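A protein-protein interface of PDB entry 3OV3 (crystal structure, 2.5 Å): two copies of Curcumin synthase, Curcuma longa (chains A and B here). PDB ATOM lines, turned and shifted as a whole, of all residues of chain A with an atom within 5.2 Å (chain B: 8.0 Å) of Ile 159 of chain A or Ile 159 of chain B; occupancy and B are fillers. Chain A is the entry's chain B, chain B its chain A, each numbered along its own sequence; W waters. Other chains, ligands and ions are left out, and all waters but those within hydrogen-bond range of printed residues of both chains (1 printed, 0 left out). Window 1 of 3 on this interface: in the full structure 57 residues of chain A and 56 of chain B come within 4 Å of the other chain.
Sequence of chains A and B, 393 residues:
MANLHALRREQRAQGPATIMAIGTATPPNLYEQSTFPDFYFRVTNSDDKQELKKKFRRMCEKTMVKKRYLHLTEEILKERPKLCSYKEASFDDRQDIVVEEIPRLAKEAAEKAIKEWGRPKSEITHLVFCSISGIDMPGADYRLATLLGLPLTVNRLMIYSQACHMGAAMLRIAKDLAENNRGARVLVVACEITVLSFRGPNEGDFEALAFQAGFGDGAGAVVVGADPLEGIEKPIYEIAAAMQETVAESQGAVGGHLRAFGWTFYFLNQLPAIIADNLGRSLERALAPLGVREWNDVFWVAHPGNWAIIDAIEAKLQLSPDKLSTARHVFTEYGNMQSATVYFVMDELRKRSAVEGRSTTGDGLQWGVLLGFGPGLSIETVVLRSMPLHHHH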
ATOM      1  N   VAL A 128     -24.474  10.926  -8.066  1.00  0.00           N
ATOM      2  CA  VAL A 128     -25.185  12.090  -8.561  1.00  0.00           C
ATOM      3  C   VAL A 128     -24.989  13.239  -7.571  1.00  0.00           C
ATOM      4  O   VAL A 128     -25.374  13.155  -6.386  1.00  0.00           O
ATOM      5  CB  VAL A 128     -26.690  11.823  -8.751  1.00  0.00           C
ATOM      6  CG1 VAL A 128     -27.384  13.109  -9.160  1.00  0.00           C
ATOM      7  CG2 VAL A 128     -26.912  10.718  -9.789  1.00  0.00           C
ATOM      8  N   PHE A 129     -24.391  14.310  -8.095  1.00  0.00           N
ATOM      9  CA  PHE A 129     -23.909  15.419  -7.309  1.00  0.00           C
ATOM     10  C   PHE A 129     -24.315  16.747  -7.914  1.00  0.00           C
ATOM     11  O   PHE A 129     -24.027  16.999  -9.089  1.00  0.00           O
ATOM     12  CB  PHE A 129     -22.385  15.354  -7.286  1.00  0.00           C
ATOM     13  CG  PHE A 129     -21.734  16.394  -6.397  1.00  0.00           C
ATOM     14  CD1 PHE A 129     -22.414  16.953  -5.328  1.00  0.00           C
ATOM     15  CD2 PHE A 129     -20.401  16.744  -6.589  1.00  0.00           C
ATOM     16  CE1 PHE A 129     -21.776  17.895  -4.483  1.00  0.00           C
ATOM     17  CE2 PHE A 129     -19.753  17.676  -5.758  1.00  0.00           C
ATOM     18  CZ  PHE A 129     -20.445  18.248  -4.721  1.00  0.00           C
ATOM     19  N   CYS A 130     -24.926  17.616  -7.106  1.00  0.00           N
ATOM     20  CA  CYS A 130     -25.321  18.962  -7.574  1.00  0.00           C
ATOM     21  C   CYS A 130     -24.847  20.081  -6.681  1.00  0.00           C
ATOM     22  O   CYS A 130     -24.751  19.937  -5.444  1.00  0.00           O
ATOM     23  CB  CYS A 130     -26.831  19.092  -7.750  1.00  0.00           C
ATOM     24  SG  CYS A 130     -27.748  19.039  -6.156  1.00  0.00           S
ATOM     25  N   SER A 131     -24.554  21.203  -7.341  1.00  0.00           N
ATOM     26  CA  SER A 131     -24.224  22.452  -6.697  1.00  0.00           C
ATOM     27  C   SER A 131     -24.503  23.559  -7.670  1.00  0.00           C
ATOM     28  O   SER A 131     -24.354  23.371  -8.840  1.00  0.00           O
ATOM     29  CB  SER A 131     -22.739  22.500  -6.325  1.00  0.00           C
ATOM     30  OG  SER A 131     -22.500  23.636  -5.503  1.00  0.00           O
ATOM     31  N   LEU A 157     -22.387  11.666 -12.333  1.00  0.00           N
ATOM     32  CA  LEU A 157     -23.138  12.749 -12.926  1.00  0.00           C
ATOM     33  C   LEU A 157     -23.068  14.005 -12.042  1.00  0.00           C
ATOM     34  O   LEU A 157     -23.565  14.020 -10.900  1.00  0.00           O
ATOM     35  CB  LEU A 157     -24.590  12.318 -13.107  1.00  0.00           C
ATOM     36  CG  LEU A 157     -25.532  13.349 -13.721  1.00  0.00           C
ATOM     37  CD1 LEU A 157     -24.984  13.781 -15.067  1.00  0.00           C
ATOM     38  CD2 LEU A 157     -26.945  12.753 -13.848  1.00  0.00           C
ATOM     39  N   MET A 158     -22.438  15.046 -12.570  1.00  0.00           N
ATOM     40  CA  MET A 158     -22.531  16.380 -11.988  1.00  0.00           C
ATOM     41  C   MET A 158     -23.678  17.224 -12.566  1.00  0.00           C
ATOM     42  O   MET A 158     -23.827  17.347 -13.782  1.00  0.00           O
ATOM     43  CB  MET A 158     -21.239  17.155 -12.185  1.00  0.00           C
ATOM     44  CG  MET A 158     -21.270  18.437 -11.453  1.00  0.00           C
ATOM     45  SD  MET A 158     -20.816  18.178  -9.727  1.00  0.00           S
ATOM     46  CE  MET A 158     -21.814  19.489  -8.990  1.00  0.00           C
ATOM     47  N   ILE A 159     -24.456  17.833 -11.681  1.00  0.00           N
ATOM     48  CA  ILE A 159     -25.429  18.820 -12.071  1.00  0.00           C
ATOM     49  C   ILE A 159     -25.148  20.188 -11.439  1.00  0.00           C
ATOM     50  O   ILE A 159     -25.468  20.445 -10.282  1.00  0.00           O
ATOM     51  CB  ILE A 159     -26.838  18.314 -11.741  1.00  0.00           C
ATOM     52  CG1 ILE A 159     -27.011  16.919 -12.362  1.00  0.00           C
ATOM     53  CG2 ILE A 159     -27.899  19.309 -12.201  1.00  0.00           C
ATOM     54  CD1 ILE A 159     -27.982  16.096 -11.652  1.00  0.00           C
ATOM     55  N   TYR A 160     -24.582  21.072 -12.240  1.00  0.00           N
ATOM     56  CA  TYR A 160     -24.253  22.436 -11.870  1.00  0.00           C
ATOM     57  C   TYR A 160     -25.414  23.414 -12.045  1.00  0.00           C
ATOM     58  O   TYR A 160     -26.199  23.308 -13.001  1.00  0.00           O
ATOM     59  CB  TYR A 160     -23.104  22.927 -12.769  1.00  0.00           C
ATOM     60  CG  TYR A 160     -21.713  22.465 -12.386  1.00  0.00           C
ATOM     61  CD1 TYR A 160     -21.163  22.736 -11.106  1.00  0.00           C
ATOM     62  CD2 TYR A 160     -20.918  21.786 -13.312  1.00  0.00           C
ATOM     63  CE1 TYR A 160     -19.863  22.309 -10.783  1.00  0.00           C
ATOM     64  CE2 TYR A 160     -19.653  21.377 -13.004  1.00  0.00           C
ATOM     65  CZ  TYR A 160     -19.124  21.640 -11.754  1.00  0.00           C
ATOM     66  OH  TYR A 160     -17.837  21.214 -11.509  1.00  0.00           O
ATOM     67  N   SER A 161     -25.496  24.378 -11.126  1.00  0.00           N
ATOM     68  CA  SER A 161     -26.187  25.660 -11.351  1.00  0.00           C
ATOM     69  C   SER A 161     -27.715  25.619 -11.596  1.00  0.00           C
ATOM     70  O   SER A 161     -28.277  26.489 -12.243  1.00  0.00           O
ATOM     71  CB  SER A 161     -25.479  26.456 -12.462  1.00  0.00           C
ATOM     72  OG  SER A 161     -24.150  26.767 -12.085  1.00  0.00           O
ATOM     73  N   GLN A 162     -28.373  24.602 -11.068  1.00  0.00           N
ATOM     74  CA  GLN A 162     -29.816  24.594 -10.892  1.00  0.00           C
ATOM     75  C   GLN A 162     -30.070  25.053  -9.470  1.00  0.00           C
ATOM     76  O   GLN A 162     -29.200  24.930  -8.587  1.00  0.00           O
ATOM     77  CB  GLN A 162     -30.341  23.188 -11.107  1.00  0.00           C
ATOM     78  CG  GLN A 162     -29.730  22.510 -12.353  1.00  0.00           C
ATOM     79  CD  GLN A 162     -30.228  23.156 -13.623  1.00  0.00           C
ATOM     80  OE1 GLN A 162     -31.438  23.178 -13.879  1.00  0.00           O
ATOM     81  NE2 GLN A 162     -29.308  23.716 -14.412  1.00  0.00           N
ATOM     82  N   MET A 166     -33.201  21.388  -6.913  1.00  0.00           N
ATOM     83  CA  MET A 166     -32.307  20.333  -7.401  1.00  0.00           C
ATOM     84  C   MET A 166     -32.063  19.230  -6.361  1.00  0.00           C
ATOM     85  O   MET A 166     -31.778  18.065  -6.714  1.00  0.00           O
ATOM     86  CB  MET A 166     -30.974  20.918  -7.917  1.00  0.00           C
ATOM     87  CG  MET A 166     -30.241  19.962  -8.826  1.00  0.00           C
ATOM     88  SD  MET A 166     -31.274  19.584 -10.282  1.00  0.00           S
ATOM     89  CE  MET A 166     -30.898  17.840 -10.492  1.00  0.00           C
ATOM     90  N   MET A 170     -32.771  15.354  -7.570  1.00  0.00           N
ATOM     91  CA  MET A 170     -31.797  14.297  -7.635  1.00  0.00           C
ATOM     92  C   MET A 170     -32.462  12.990  -7.266  1.00  0.00           C
ATOM     93  O   MET A 170     -32.256  11.963  -7.949  1.00  0.00           O
ATOM     94  CB  MET A 170     -30.585  14.618  -6.766  1.00  0.00           C
ATOM     95  CG  MET A 170     -29.640  15.630  -7.431  1.00  0.00           C
ATOM     96  SD  MET A 170     -28.031  15.676  -6.620  1.00  0.00           S
ATOM     97  CE  MET A 170     -28.499  16.053  -4.913  1.00  0.00           C
ATOM     98  N   ILE A 173     -33.963  11.469 -10.181  1.00  0.00           N
ATOM     99  CA  ILE A 173     -33.015  10.748 -11.030  1.00  0.00           C
ATOM    100  C   ILE A 173     -32.517   9.442 -10.402  1.00  0.00           C
ATOM    101  O   ILE A 173     -32.447   8.419 -11.072  1.00  0.00           O
ATOM    102  CB  ILE A 173     -31.788  11.598 -11.409  1.00  0.00           C
ATOM    103  CG1 ILE A 173     -32.211  12.952 -11.991  1.00  0.00           C
ATOM    104  CG2 ILE A 173     -30.906  10.834 -12.402  1.00  0.00           C
ATOM    105  CD1 ILE A 173     -31.050  13.978 -12.055  1.00  0.00           C
ATOM    106  N   LEU B 127     -37.068  15.523 -20.892  1.00  0.00           N
ATOM    107  CA  LEU B 127     -36.019  16.181 -21.645  1.00  0.00           C
ATOM    108  C   LEU B 127     -34.730  16.190 -20.824  1.00  0.00           C
ATOM    109  O   LEU B 127     -34.742  16.584 -19.667  1.00  0.00           O
ATOM    110  CB  LEU B 127     -36.412  17.613 -21.968  1.00  0.00           C
ATOM    111  CG  LEU B 127     -35.308  18.517 -22.536  1.00  0.00           C
ATOM    112  CD1 LEU B 127     -35.039  18.181 -23.978  1.00  0.00           C
ATOM    113  CD2 LEU B 127     -35.646  20.000 -22.373  1.00  0.00           C
ATOM    114  N   VAL B 128     -33.643  15.747 -21.453  1.00  0.00           N
ATOM    115  CA  VAL B 128     -32.318  15.736 -20.895  1.00  0.00           C
ATOM    116  C   VAL B 128     -31.449  16.500 -21.893  1.00  0.00           C
ATOM    117  O   VAL B 128     -31.358  16.139 -23.072  1.00  0.00           O
ATOM    118  CB  VAL B 128     -31.765  14.272 -20.671  1.00  0.00           C
ATOM    119  CG1 VAL B 128     -30.278  14.283 -20.186  1.00  0.00           C
ATOM    120  CG2 VAL B 128     -32.608  13.508 -19.658  1.00  0.00           C
ATOM    121  N   PHE B 129     -30.805  17.555 -21.406  1.00  0.00           N
ATOM    122  CA  PHE B 129     -30.173  18.566 -22.259  1.00  0.00           C
ATOM    123  C   PHE B 129     -28.814  18.922 -21.658  1.00  0.00           C
ATOM    124  O   PHE B 129     -28.713  19.230 -20.455  1.00  0.00           O
ATOM    125  CB  PHE B 129     -31.098  19.791 -22.314  1.00  0.00           C
ATOM    126  CG  PHE B 129     -30.600  20.937 -23.173  1.00  0.00           C
ATOM    127  CD1 PHE B 129     -29.671  20.747 -24.191  1.00  0.00           C
ATOM    128  CD2 PHE B 129     -31.134  22.202 -22.998  1.00  0.00           C
ATOM    129  CE1 PHE B 129     -29.237  21.807 -24.988  1.00  0.00           C
ATOM    130  CE2 PHE B 129     -30.714  23.274 -23.797  1.00  0.00           C
ATOM    131  CZ  PHE B 129     -29.770  23.063 -24.805  1.00  0.00           C
ATOM    132  N   CYS B 130     -27.771  18.823 -22.479  1.00  0.00           N
ATOM    133  CA  CYS B 130     -26.437  19.200 -22.052  1.00  0.00           C
ATOM    134  C   CYS B 130     -25.810  20.252 -22.941  1.00  0.00           C
ATOM    135  O   CYS B 130     -26.024  20.287 -24.147  1.00  0.00           O
ATOM    136  CB  CYS B 130     -25.508  17.975 -21.947  1.00  0.00           C
ATOM    137  SG  CYS B 130     -24.820  17.334 -23.501  1.00  0.00           S
ATOM    138  N   SER B 131     -25.007  21.098 -22.317  1.00  0.00           N
ATOM    139  CA  SER B 131     -24.181  22.074 -23.003  1.00  0.00           C
ATOM    140  C   SER B 131     -23.111  22.488 -22.006  1.00  0.00           C
ATOM    141  O   SER B 131     -23.331  22.421 -20.780  1.00  0.00           O
ATOM    142  CB  SER B 131     -24.973  23.326 -23.401  1.00  0.00           C
ATOM    143  OG  SER B 131     -24.110  24.230 -24.080  1.00  0.00           O
ATOM    144  N   ILE B 132     -21.966  22.904 -22.552  1.00  0.00           N
ATOM    145  CA  ILE B 132     -20.947  23.572 -21.789  1.00  0.00           C
ATOM    146  C   ILE B 132     -21.454  24.938 -21.354  1.00  0.00           C
ATOM    147  O   ILE B 132     -21.051  25.431 -20.291  1.00  0.00           O
ATOM    148  CB  ILE B 132     -19.658  23.751 -22.617  1.00  0.00           C
ATOM    149  CG1 ILE B 132     -18.934  22.417 -22.727  1.00  0.00           C
ATOM    150  CG2 ILE B 132     -18.749  24.740 -21.945  1.00  0.00           C
ATOM    151  CD1 ILE B 132     -17.766  22.421 -23.705  1.00  0.00           C
ATOM    152  N   SER B 133     -22.358  25.521 -22.139  1.00  0.00           N
ATOM    153  CA  SER B 133     -22.635  26.974 -22.085  1.00  0.00           C
ATOM    154  C   SER B 133     -24.071  27.356 -21.782  1.00  0.00           C
ATOM    155  O   SER B 133     -24.989  26.546 -21.963  1.00  0.00           O
ATOM    156  CB  SER B 133     -22.299  27.593 -23.446  1.00  0.00           C
ATOM    157  OG  SER B 133     -20.951  27.326 -23.791  1.00  0.00           O
ATOM    158  N   ILE B 135     -25.375  29.213 -18.851  1.00  0.00           N
ATOM    159  CA  ILE B 135     -25.786  29.190 -17.475  1.00  0.00           C
ATOM    160  C   ILE B 135     -26.575  30.453 -17.115  1.00  0.00           C
ATOM    161  O   ILE B 135     -26.138  31.578 -17.403  1.00  0.00           O
ATOM    162  CB  ILE B 135     -24.579  28.967 -16.565  1.00  0.00           C
ATOM    163  CG1 ILE B 135     -23.993  27.587 -16.848  1.00  0.00           C
ATOM    164  CG2 ILE B 135     -24.979  29.013 -15.100  1.00  0.00           C
ATOM    165  CD1 ILE B 135     -22.814  27.228 -15.969  1.00  0.00           C
ATOM    166  N   ALA B 140     -31.164  26.583 -19.506  1.00  0.00           N
ATOM    167  CA  ALA B 140     -31.373  26.346 -20.930  1.00  0.00           C
ATOM    168  C   ALA B 140     -32.417  25.246 -21.200  1.00  0.00           C
ATOM    169  O   ALA B 140     -33.056  25.226 -22.265  1.00  0.00           O
ATOM    170  CB  ALA B 140     -30.036  26.065 -21.637  1.00  0.00           C
ATOM    171  N   ASP B 141     -32.605  24.346 -20.230  1.00  0.00           N
ATOM    172  CA  ASP B 141     -33.664  23.333 -20.345  1.00  0.00           C
ATOM    173  C   ASP B 141     -35.031  24.022 -20.406  1.00  0.00           C
ATOM    174  O   ASP B 141     -35.831  23.769 -21.311  1.00  0.00           O
ATOM    175  CB  ASP B 141     -33.577  22.286 -19.228  1.00  0.00           C
ATOM    176  CG  ASP B 141     -33.687  22.888 -17.815  1.00  0.00           C
ATOM    177  OD1 ASP B 141     -33.107  23.952 -17.539  1.00  0.00           O
ATOM    178  OD2 ASP B 141     -34.331  22.259 -16.954  1.00  0.00           O
ATOM    179  N   ARG B 156     -37.574  17.761 -16.790  1.00  0.00           N
ATOM    180  CA  ARG B 156     -36.469  18.430 -17.401  1.00  0.00           C
ATOM    181  C   ARG B 156     -35.227  18.216 -16.550  1.00  0.00           C
ATOM    182  O   ARG B 156     -35.279  18.244 -15.305  1.00  0.00           O
ATOM    183  CB  ARG B 156     -36.785  19.915 -17.501  1.00  0.00           C
ATOM    184  CG  ARG B 156     -38.063  20.240 -18.267  1.00  0.00           C
ATOM    185  CD  ARG B 156     -38.539  21.671 -17.985  1.00  0.00           C
ATOM    186  NE  ARG B 156     -37.467  22.427 -17.329  1.00  0.00           N
ATOM    187  CZ  ARG B 156     -37.594  23.090 -16.186  1.00  0.00           C
ATOM    188  NH1 ARG B 156     -38.771  23.164 -15.573  1.00  0.00           N
ATOM    189  NH2 ARG B 156     -36.540  23.703 -15.669  1.00  0.00           N
ATOM    190  N   LEU B 157     -34.108  17.986 -17.234  1.00  0.00           N
ATOM    191  CA  LEU B 157     -32.810  17.939 -16.595  1.00  0.00           C
ATOM    192  C   LEU B 157     -31.774  18.608 -17.482  1.00  0.00           C
ATOM    193  O   LEU B 157     -31.629  18.275 -18.655  1.00  0.00           O
ATOM    194  CB  LEU B 157     -32.430  16.498 -16.264  1.00  0.00           C
ATOM    195  CG  LEU B 157     -31.019  16.306 -15.703  1.00  0.00           C
ATOM    196  CD1 LEU B 157     -30.852  16.933 -14.309  1.00  0.00           C
ATOM    197  CD2 LEU B 157     -30.631  14.842 -15.710  1.00  0.00           C
ATOM    198  N   MET B 158     -31.086  19.593 -16.910  1.00  0.00           N
ATOM    199  CA  MET B 158     -29.998  20.310 -17.582  1.00  0.00           C
ATOM    200  C   MET B 158     -28.665  19.857 -17.031  1.00  0.00           C
ATOM    201  O   MET B 158     -28.464  19.860 -15.804  1.00  0.00           O
ATOM    202  CB  MET B 158     -30.126  21.846 -17.439  1.00  0.00           C
ATOM    203  CG  MET B 158     -29.093  22.633 -18.335  1.00  0.00           C
ATOM    204  SD  MET B 158     -29.568  22.569 -20.087  1.00  0.00           S
ATOM    205  CE  MET B 158     -28.007  22.553 -20.970  1.00  0.00           C
ATOM    206  N   ILE B 159     -27.749  19.489 -17.928  1.00  0.00           N
ATOM    207  CA  ILE B 159     -26.383  19.181 -17.525  1.00  0.00           C
ATOM    208  C   ILE B 159     -25.437  20.198 -18.128  1.00  0.00           C
ATOM    209  O   ILE B 159     -25.125  20.114 -19.303  1.00  0.00           O
ATOM    210  CB  ILE B 159     -25.942  17.745 -17.963  1.00  0.00           C
ATOM    211  CG1 ILE B 159     -27.060  16.700 -17.713  1.00  0.00           C
ATOM    212  CG2 ILE B 159     -24.618  17.353 -17.263  1.00  0.00           C
ATOM    213  CD1 ILE B 159     -27.361  16.481 -16.201  1.00  0.00           C
ATOM    214  N   TYR B 160     -24.995  21.160 -17.327  1.00  0.00           N
ATOM    215  CA  TYR B 160     -24.057  22.208 -17.758  1.00  0.00           C
ATOM    216  C   TYR B 160     -22.552  21.884 -17.594  1.00  0.00           C
ATOM    217  O   TYR B 160     -22.145  21.286 -16.606  1.00  0.00           O
ATOM    218  CB  TYR B 160     -24.308  23.516 -16.984  1.00  0.00           C
ATOM    219  CG  TYR B 160     -25.464  24.373 -17.434  1.00  0.00           C
ATOM    220  CD1 TYR B 160     -25.569  24.828 -18.752  1.00  0.00           C
ATOM    221  CD2 TYR B 160     -26.434  24.789 -16.515  1.00  0.00           C
ATOM    222  CE1 TYR B 160     -26.643  25.641 -19.143  1.00  0.00           C
ATOM    223  CE2 TYR B 160     -27.480  25.595 -16.878  1.00  0.00           C
ATOM    224  CZ  TYR B 160     -27.594  26.025 -18.184  1.00  0.00           C
ATOM    225  OH  TYR B 160     -28.669  26.825 -18.526  1.00  0.00           O
ATOM    226  N   SER B 161     -21.740  22.353 -18.539  1.00  0.00           N
ATOM    227  CA  SER B 161     -20.291  22.484 -18.351  1.00  0.00           C
ATOM    228  C   SER B 161     -19.522  21.175 -18.170  1.00  0.00           C
ATOM    229  O   SER B 161     -18.528  21.167 -17.480  1.00  0.00           O
ATOM    230  CB  SER B 161     -19.949  23.437 -17.181  1.00  0.00           C
ATOM    231  OG  SER B 161     -20.483  24.746 -17.366  1.00  0.00           O
ATOM    232  N   GLN B 162     -20.010  20.084 -18.755  1.00  0.00           N
ATOM    233  CA  GLN B 162     -19.307  18.796 -18.856  1.00  0.00           C
ATOM    234  C   GLN B 162     -18.872  18.742 -20.282  1.00  0.00           C
ATOM    235  O   GLN B 162     -19.571  19.281 -21.163  1.00  0.00           O
ATOM    236  CB  GLN B 162     -20.279  17.631 -18.653  1.00  0.00           C
ATOM    237  CG  GLN B 162     -21.180  17.784 -17.440  1.00  0.00           C
ATOM    238  CD  GLN B 162     -20.397  17.799 -16.150  1.00  0.00           C
ATOM    239  OE1 GLN B 162     -20.428  18.786 -15.419  1.00  0.00           O
ATOM    240  NE2 GLN B 162     -19.651  16.724 -15.882  1.00  0.00           N
ATOM    241  N   ALA B 163     -17.764  18.112 -20.594  1.00  0.00           N
ATOM    242  CA  ALA B 163     -17.290  18.388 -21.943  1.00  0.00           C
ATOM    243  C   ALA B 163     -17.768  17.390 -22.966  1.00  0.00           C
ATOM    244  O   ALA B 163     -18.960  17.064 -23.010  1.00  0.00           O
ATOM    245  CB  ALA B 163     -15.802  18.564 -21.987  1.00  0.00           C
ATOM    246  N   MET B 166     -20.102  14.180 -22.632  1.00  0.00           N
ATOM    247  CA  MET B 166     -21.439  14.315 -22.107  1.00  0.00           C
ATOM    248  C   MET B 166     -22.479  13.851 -23.114  1.00  0.00           C
ATOM    249  O   MET B 166     -23.554  13.392 -22.726  1.00  0.00           O
ATOM    250  CB  MET B 166     -21.707  15.747 -21.620  1.00  0.00           C
ATOM    251  CG  MET B 166     -22.927  15.832 -20.684  1.00  0.00           C
ATOM    252  SD  MET B 166     -22.917  14.695 -19.238  1.00  0.00           S
ATOM    253  CE  MET B 166     -24.616  14.086 -19.272  1.00  0.00           C
ATOM    254  N   ALA B 169     -22.784  10.362 -22.437  1.00  0.00           N
ATOM    255  CA  ALA B 169     -23.321  10.187 -21.084  1.00  0.00           C
ATOM    256  C   ALA B 169     -24.848  10.378 -21.072  1.00  0.00           C
ATOM    257  O   ALA B 169     -25.580   9.665 -20.414  1.00  0.00           O
ATOM    258  CB  ALA B 169     -22.639  11.141 -20.111  1.00  0.00           C
ATOM    259  N   MET B 170     -25.342  11.322 -21.840  1.00  0.00           N
ATOM    260  CA  MET B 170     -26.792  11.483 -21.958  1.00  0.00           C
ATOM    261  C   MET B 170     -27.503  10.208 -22.386  1.00  0.00           C
ATOM    262  O   MET B 170     -28.579   9.900 -21.905  1.00  0.00           O
ATOM    263  CB  MET B 170     -27.095  12.637 -22.893  1.00  0.00           C
ATOM    264  CG  MET B 170     -26.934  14.016 -22.197  1.00  0.00           C
ATOM    265  SD  MET B 170     -27.730  15.259 -23.218  1.00  0.00           S
ATOM    266  CE  MET B 170     -26.881  14.959 -24.794  1.00  0.00           C
ATOM    267  N   ILE B 173     -27.960   8.159 -19.238  1.00  0.00           N
ATOM    268  CA  ILE B 173     -29.102   8.586 -18.438  1.00  0.00           C
ATOM    269  C   ILE B 173     -30.438   8.235 -19.116  1.00  0.00           C
ATOM    270  O   ILE B 173     -31.287   7.577 -18.535  1.00  0.00           O
ATOM    271  CB  ILE B 173     -29.002  10.089 -18.131  1.00  0.00           C
ATOM    272  CG1 ILE B 173     -27.754  10.368 -17.275  1.00  0.00           C
ATOM    273  CG2 ILE B 173     -30.270  10.607 -17.423  1.00  0.00           C
ATOM    274  CD1 ILE B 173     -27.230  11.816 -17.455  1.00  0.00           C
ATOM    275  N   VAL B 189     -30.712  16.078 -25.836  1.00  0.00           N
ATOM    276  CA  VAL B 189     -30.189  17.119 -26.706  1.00  0.00           C
ATOM    277  C   VAL B 189     -28.833  17.617 -26.209  1.00  0.00           C
ATOM    278  O   VAL B 189     -28.640  17.879 -24.983  1.00  0.00           O
ATOM    279  CB  VAL B 189     -31.226  18.330 -26.935  1.00  0.00           C
ATOM    280  CG1 VAL B 189     -30.732  19.294 -28.001  1.00  0.00           C
ATOM    281  CG2 VAL B 189     -32.673  17.850 -27.303  1.00  0.00           C
ATOM    282  N   CYS B 191     -25.993  20.599 -27.388  1.00  0.00           N
ATOM    283  CA  CYS B 191     -25.761  21.781 -28.199  1.00  0.00           C
ATOM    284  C   CYS B 191     -24.525  22.433 -27.678  1.00  0.00           C
ATOM    285  O   CYS B 191     -24.369  22.580 -26.444  1.00  0.00           O
ATOM    286  CB  CYS B 191     -26.923  22.744 -28.045  1.00  0.00           C
ATOM    287  SG  CYS B 191     -26.748  24.236 -29.019  1.00  0.00           S
ATOM    288  N   GLU B 192     -23.620  22.802 -28.580  1.00  0.00           N
ATOM    289  CA  GLU B 192     -22.474  23.596 -28.165  1.00  0.00           C
ATOM    290  C   GLU B 192     -22.273  24.782 -29.091  1.00  0.00           C
ATOM    291  O   GLU B 192     -22.430  24.677 -30.301  1.00  0.00           O
ATOM    292  CB  GLU B 192     -21.189  22.771 -28.110  1.00  0.00           C
ATOM    293  CG  GLU B 192     -21.303  21.433 -27.438  1.00  0.00           C
ATOM    294  CD  GLU B 192     -21.270  21.468 -25.916  1.00  0.00           C
ATOM    295  OE1 GLU B 192     -21.245  22.544 -25.267  1.00  0.00           O
ATOM    296  OE2 GLU B 192     -21.257  20.373 -25.355  1.00  0.00           O
ATOM    297  N   SER B 339     -19.820  18.018 -27.097  1.00  0.00           N
ATOM    298  CA  SER B 339     -20.763  16.948 -26.737  1.00  0.00           C
ATOM    299  C   SER B 339     -21.702  16.542 -27.883  1.00  0.00           C
ATOM    300  O   SER B 339     -22.190  15.420 -27.922  1.00  0.00           O
ATOM    301  CB  SER B 339     -21.540  17.233 -25.453  1.00  0.00           C
ATOM    302  OG  SER B 339     -22.646  18.072 -25.704  1.00  0.00           O
HETATM  303  O   HOH W   1     -21.089  14.412 -15.099  1.00  0.00           O
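Of the printed residues of chain B, Ile 159 of chain A touches Leu 157, Met 158 and Ile 159. Ile 159 of chain B touches just these residues of chain A: Leu 157 (3.8 Å), Met 158 (3.6 Å) and Ile 159 (3.9 Å). Printed residues of chain B within 4 Å of Gln 162 of chain A: Met 158 and Tyr 160. Of the printed residues of chain B, Ile 173 of chain A touches Leu 157. Printed residues of chain A within 4 Å of Met 158 of chain B: Ile 159 and Gln 162. Of the printed residues of chain A, Gln 162 of chain B touches Met 158 and Tyr 160. Val 128 of chain B touches none of the printed residues of chain A. The nearest printed residue of chain A that does not touch Ile 159 of chain B is Gln 162 of chain A (5.7 Å). The nearest printed residue of chain A that does not touch Met 158 of chain B is Tyr 160 of chain A (5.0 Å).
OE1 of Gln 162 of chain B touches CB of Met 158 of chain A (3.7 Å). Leu 157 of chain B touches Ile 159 of chain A (CD1 to CD1, 3.9996 Å). Ile 159 of chain A touches Met 158 of chain B (CG2 to O, 3.7 Å). Ile 159 of chain B touches Ile 159 of chain A (CD1 to CG1, 3.9 Å). O of Tyr 160 of chain B touches CD2 of Tyr 160 of chain A (3.6 Å). Tyr 160 of chain A touches Gln 162 of chain B (CE2 to OE1, 3.6 Å). CG2 of Ile 135 of chain B touches CB of Ser 161 of chain A (3.7 Å).
Of the 26 printed residues of chain B, 7 touch a printed residue of chain A. Hydrophobic or aromatic side chains of chain B that line the printed part of chain A: Ile 135, Leu 157, Met 158, Ile 159, Tyr 160 and Ile 173. Of the 13 printed residues of chain A, 8 touch a printed residue of chain B. Among the printed residues, no Asp or Glu carboxylate lies within 4 Å of a Lys or Arg side-chain nitrogen of the other chain.
Met 158 of chain A touches Ile 159 of chain B, and with the chains exchanged Ile 159 of chain A touches Met 158 of chain B. Met 158 of chain A touches Gln 162 of chain B, and with the chains exchanged Gln 162 of chain A touches Met 158 of chain B. Ile 159 of chain A touches its own counterpart, Ile 159 of chain B. Tyr 160 of chain A touches Gln 162 of chain B, and with the chains exchanged Gln 162 of chain A touches Tyr 160 of chain B.
Water W1 bridges NE2 of Gln 162 of chain B (2.8 Å) and N of Met 158 of chain A (2.9 Å).
The backbone carbonyl oxygen (O) of Leu 127 of chain B sits at hydrogen-bond distance from the backbone NH (N) of Leu 157 of chain B (2.9 Å). The side-chain amide oxygen of Gln 162 of chain B sits close to the backbone carbonyl oxygen of Tyr 160 of chain B (3.3 Å). The backbone carbonyl oxygen (O) of Ser 131 of chain A lies within hydrogen-bond range of the backbone NH (N) of Ser 161 of chain A (2.7 Å).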
